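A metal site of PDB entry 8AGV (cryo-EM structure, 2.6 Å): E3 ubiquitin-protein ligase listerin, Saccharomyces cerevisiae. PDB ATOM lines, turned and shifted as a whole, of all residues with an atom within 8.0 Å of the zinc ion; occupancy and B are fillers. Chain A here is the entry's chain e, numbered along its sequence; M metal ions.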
ATOM      1  N   THR A1526     -25.670 -31.232   4.537  1.00  0.00           N
ATOM      2  CA  THR A1526     -24.525 -30.970   3.690  1.00  0.00           C
ATOM      3  C   THR A1526     -23.838 -29.685   4.125  1.00  0.00           C
ATOM      4  O   THR A1526     -24.492 -28.662   4.309  1.00  0.00           O
ATOM      5  CB  THR A1526     -24.913 -30.838   2.200  1.00  0.00           C
ATOM      6  OG1 THR A1526     -26.030 -29.956   2.076  1.00  0.00           O
ATOM      7  CG2 THR A1526     -25.279 -32.200   1.620  1.00  0.00           C
ATOM      8  N   CYS A1527     -22.529 -29.743   4.302  1.00  0.00           N
ATOM      9  CA  CYS A1527     -21.778 -28.547   4.681  1.00  0.00           C
ATOM     10  C   CYS A1527     -21.815 -27.545   3.537  1.00  0.00           C
ATOM     11  O   CYS A1527     -21.682 -27.927   2.373  1.00  0.00           O
ATOM     12  CB  CYS A1527     -20.346 -28.939   4.995  1.00  0.00           C
ATOM     13  SG  CYS A1527     -19.199 -27.626   5.447  1.00  0.00           S
ATOM     14  N   PRO A1528     -22.023 -26.263   3.846  1.00  0.00           N
ATOM     15  CA  PRO A1528     -21.957 -25.288   2.746  1.00  0.00           C
ATOM     16  C   PRO A1528     -20.562 -25.245   2.165  1.00  0.00           C
ATOM     17  O   PRO A1528     -20.404 -25.214   0.939  1.00  0.00           O
ATOM     18  CB  PRO A1528     -22.280 -23.964   3.434  1.00  0.00           C
ATOM     19  CG  PRO A1528     -23.028 -24.338   4.666  1.00  0.00           C
ATOM     20  CD  PRO A1528     -22.433 -25.643   5.112  1.00  0.00           C
ATOM     21  N   THR A1529     -19.552 -25.228   3.027  1.00  0.00           N
ATOM     22  CA  THR A1529     -18.171 -25.161   2.564  1.00  0.00           C
ATOM     23  C   THR A1529     -17.695 -26.391   1.801  1.00  0.00           C
ATOM     24  O   THR A1529     -17.018 -26.263   0.789  1.00  0.00           O
ATOM     25  CB  THR A1529     -17.223 -24.918   3.753  1.00  0.00           C
ATOM     26  OG1 THR A1529     -17.857 -24.043   4.688  1.00  0.00           O
ATOM     27  CG2 THR A1529     -15.911 -24.309   3.266  1.00  0.00           C
ATOM     28  N   CYS A1530     -18.067 -27.578   2.272  1.00  0.00           N
ATOM     29  CA  CYS A1530     -17.576 -28.795   1.630  1.00  0.00           C
ATOM     30  C   CYS A1530     -18.703 -29.726   1.186  1.00  0.00           C
ATOM     31  O   CYS A1530     -19.732 -29.819   1.832  1.00  0.00           O
ATOM     32  CB  CYS A1530     -16.550 -29.520   2.501  1.00  0.00           C
ATOM     33  SG  CYS A1530     -17.159 -30.252   4.038  1.00  0.00           S
ATOM     34  N   LYS A1531     -18.486 -30.448   0.092  1.00  0.00           N
ATOM     35  CA  LYS A1531     -19.526 -31.312  -0.457  1.00  0.00           C
ATOM     36  C   LYS A1531     -19.874 -32.508   0.410  1.00  0.00           C
ATOM     37  O   LYS A1531     -20.897 -33.162   0.186  1.00  0.00           O
ATOM     38  CB  LYS A1531     -19.137 -31.787  -1.861  1.00  0.00           C
ATOM     39  CG  LYS A1531     -18.955 -30.665  -2.871  1.00  0.00           C
ATOM     40  CD  LYS A1531     -18.567 -31.207  -4.230  1.00  0.00           C
ATOM     41  CE  LYS A1531     -18.352 -30.076  -5.229  1.00  0.00           C
ATOM     42  NZ  LYS A1531     -17.939 -30.586  -6.566  1.00  0.00           N
ATOM     43  N   ASN A1532     -19.044 -32.812   1.406  1.00  0.00           N
ATOM     44  CA  ASN A1532     -19.276 -33.996   2.212  1.00  0.00           C
ATOM     45  C   ASN A1532     -20.627 -34.014   2.897  1.00  0.00           C
ATOM     46  O   ASN A1532     -21.104 -32.983   3.376  1.00  0.00           O
ATOM     47  CB  ASN A1532     -18.161 -34.134   3.246  1.00  0.00           C
ATOM     48  CG  ASN A1532     -16.781 -34.180   2.611  1.00  0.00           C
ATOM     49  OD1 ASN A1532     -16.100 -33.159   2.524  1.00  0.00           O
ATOM     50  ND2 ASN A1532     -16.377 -35.353   2.152  1.00  0.00           N
ATOM     51  N   PHE A1534     -23.201 -35.277   5.864  1.00  0.00           N
ATOM     52  CA  PHE A1534     -23.163 -35.736   7.242  1.00  0.00           C
ATOM     53  C   PHE A1534     -24.537 -36.146   7.712  1.00  0.00           C
ATOM     54  O   PHE A1534     -25.519 -35.489   7.381  1.00  0.00           O
ATOM     55  CB  PHE A1534     -22.661 -34.627   8.170  1.00  0.00           C
ATOM     56  CG  PHE A1534     -21.361 -34.005   7.742  1.00  0.00           C
ATOM     57  CD1 PHE A1534     -20.162 -34.567   8.121  1.00  0.00           C
ATOM     58  CD2 PHE A1534     -21.348 -32.843   6.988  1.00  0.00           C
ATOM     59  CE1 PHE A1534     -18.961 -33.987   7.751  1.00  0.00           C
ATOM     60  CE2 PHE A1534     -20.159 -32.268   6.612  1.00  0.00           C
ATOM     61  CZ  PHE A1534     -18.961 -32.844   6.989  1.00  0.00           C
ATOM     62  N   LEU A1539     -23.597 -34.990  12.914  1.00  0.00           N
ATOM     63  CA  LEU A1539     -23.179 -33.593  12.843  1.00  0.00           C
ATOM     64  C   LEU A1539     -23.505 -32.862  14.128  1.00  0.00           C
ATOM     65  O   LEU A1539     -22.692 -32.100  14.638  1.00  0.00           O
ATOM     66  CB  LEU A1539     -23.858 -32.897  11.670  1.00  0.00           C
ATOM     67  CG  LEU A1539     -23.282 -31.550  11.258  1.00  0.00           C
ATOM     68  CD1 LEU A1539     -21.824 -31.701  10.865  1.00  0.00           C
ATOM     69  CD2 LEU A1539     -24.088 -30.955  10.121  1.00  0.00           C
ATOM     70  N   THR A1550     -19.429 -25.981  13.990  1.00  0.00           N
ATOM     71  CA  THR A1550     -18.159 -26.162  13.308  1.00  0.00           C
ATOM     72  C   THR A1550     -18.117 -27.488  12.558  1.00  0.00           C
ATOM     73  O   THR A1550     -18.349 -28.533  13.144  1.00  0.00           O
ATOM     74  CB  THR A1550     -16.981 -26.119  14.289  1.00  0.00           C
ATOM     75  OG1 THR A1550     -17.256 -26.980  15.412  1.00  0.00           O
ATOM     76  CG2 THR A1550     -16.749 -24.703  14.795  1.00  0.00           C
ATOM     77  N   CYS A1551     -17.802 -27.442  11.273  1.00  0.00           N
ATOM     78  CA  CYS A1551     -17.724 -28.663  10.475  1.00  0.00           C
ATOM     79  C   CYS A1551     -16.577 -29.552  10.953  1.00  0.00           C
ATOM     80  O   CYS A1551     -15.494 -29.064  11.231  1.00  0.00           O
ATOM     81  CB  CYS A1551     -17.519 -28.297   9.009  1.00  0.00           C
ATOM     82  SG  CYS A1551     -17.324 -29.669   7.861  1.00  0.00           S
ATOM     83  N   PRO A1552     -16.821 -30.863  11.060  1.00  0.00           N
ATOM     84  CA  PRO A1552     -15.693 -31.723  11.434  1.00  0.00           C
ATOM     85  C   PRO A1552     -14.592 -31.774  10.387  1.00  0.00           C
ATOM     86  O   PRO A1552     -13.418 -31.648  10.726  1.00  0.00           O
ATOM     87  CB  PRO A1552     -16.338 -33.119  11.551  1.00  0.00           C
ATOM     88  CG  PRO A1552     -17.809 -32.898  11.586  1.00  0.00           C
ATOM     89  CD  PRO A1552     -18.081 -31.615  10.877  1.00  0.00           C
ATOM     90  N   LEU A1553     -14.965 -31.947   9.126  1.00  0.00           N
ATOM     91  CA  LEU A1553     -13.983 -32.034   8.054  1.00  0.00           C
ATOM     92  C   LEU A1553     -13.228 -30.754   7.762  1.00  0.00           C
ATOM     93  O   LEU A1553     -12.025 -30.779   7.510  1.00  0.00           O
ATOM     94  CB  LEU A1553     -14.591 -32.600   6.772  1.00  0.00           C
ATOM     95  CG  LEU A1553     -14.765 -34.127   6.788  1.00  0.00           C
ATOM     96  CD1 LEU A1553     -14.616 -34.662   5.377  1.00  0.00           C
ATOM     97  CD2 LEU A1553     -13.727 -34.770   7.691  1.00  0.00           C
ATOM     98  N   CYS A1554     -13.927 -29.620   7.801  1.00  0.00           N
ATOM     99  CA  CYS A1554     -13.283 -28.360   7.440  1.00  0.00           C
ATOM    100  C   CYS A1554     -13.446 -27.286   8.509  1.00  0.00           C
ATOM    101  O   CYS A1554     -14.383 -27.325   9.290  1.00  0.00           O
ATOM    102  CB  CYS A1554     -13.798 -27.858   6.095  1.00  0.00           C
ATOM    103  SG  CYS A1554     -15.433 -27.079   6.141  1.00  0.00           S
ATOM    104  N   ARG A1555     -12.527 -26.340   8.534  1.00  0.00           N
ATOM    105  CA  ARG A1555     -12.567 -25.284   9.552  1.00  0.00           C
ATOM    106  C   ARG A1555     -13.813 -24.419   9.469  1.00  0.00           C
ATOM    107  O   ARG A1555     -14.364 -24.013  10.494  1.00  0.00           O
ATOM    108  CB  ARG A1555     -11.313 -24.412   9.480  1.00  0.00           C
ATOM    109  CG  ARG A1555     -10.118 -24.958  10.252  1.00  0.00           C
ATOM    110  CD  ARG A1555      -9.406 -26.057   9.487  1.00  0.00           C
ATOM    111  NE  ARG A1555      -8.603 -26.894  10.367  1.00  0.00           N
ATOM    112  CZ  ARG A1555      -9.023 -28.037  10.903  1.00  0.00           C
ATOM    113  NH1 ARG A1555     -10.250 -28.483  10.657  1.00  0.00           N
ATOM    114  NH2 ARG A1555      -8.225 -28.733  11.700  1.00  0.00           N
ATOM    115  N   SER A1556     -14.274 -24.122   8.255  1.00  0.00           N
ATOM    116  CA  SER A1556     -15.402 -23.201   8.098  1.00  0.00           C
ATOM    117  C   SER A1556     -16.702 -23.663   8.735  1.00  0.00           C
ATOM    118  O   SER A1556     -17.027 -24.845   8.717  1.00  0.00           O
ATOM    119  CB  SER A1556     -15.604 -22.862   6.630  1.00  0.00           C
ATOM    120  OG  SER A1556     -16.718 -21.993   6.462  1.00  0.00           O
ATOM    121  N   GLU A1557     -17.454 -22.720   9.281  1.00  0.00           N
ATOM    122  CA  GLU A1557     -18.704 -23.048   9.978  1.00  0.00           C
ATOM    123  C   GLU A1557     -19.896 -23.496   9.144  1.00  0.00           C
ATOM    124  O   GLU A1557     -20.003 -23.147   7.973  1.00  0.00           O
ATOM    125  CB  GLU A1557     -19.131 -21.842  10.833  1.00  0.00           C
ATOM    126  N   ILE A1558     -20.795 -24.271   9.761  1.00  0.00           N
ATOM    127  CA  ILE A1558     -22.009 -24.696   9.073  1.00  0.00           C
ATOM    128  C   ILE A1558     -23.174 -24.001   9.776  1.00  0.00           C
ATOM    129  O   ILE A1558     -23.296 -24.078  10.995  1.00  0.00           O
ATOM    130  CB  ILE A1558     -22.239 -26.209   9.210  1.00  0.00           C
ATOM    131  CG1 ILE A1558     -21.046 -26.993   8.662  1.00  0.00           C
ATOM    132  CG2 ILE A1558     -23.516 -26.633   8.507  1.00  0.00           C
ATOM    133  CD1 ILE A1558     -21.254 -28.490   8.712  1.00  0.00           C
HETATM  134 ZN    ZN M   1     -17.116 -28.665   5.758  1.00  0.00          ZN
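The side-chain sulfur (SG) of Cys 1527 lies close to the backbone NH (N) of Thr 1529.
The backbone NH (N) of Leu 1553 lies close to the side-chain sulfur (SG) of Cys 1551, at 3.5 Å.
The backbone carbonyl oxygen (O) of Ser 1556 lies close to the side-chain sulfur (SG) of Cys 1554, 3.8 Å away.
SG of Cys 1530 sits close to OD1 of Asn 1532 (3.4 Å).
Of the 18 residues printed, 4 come within 4 Å of the zinc ion.
The nearest printed residue that does not touch the zinc ion is Thr 1529 (4.3 Å).
The zinc ion is bound by SG of Cys 1551 (2.3 Å), SG of Cys 1530 (2.3 Å), SG of Cys 1554 (2.3 Å) and SG of Cys 1527 (2.3 Å).
The zinc ion has four donor atoms within binding distance.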
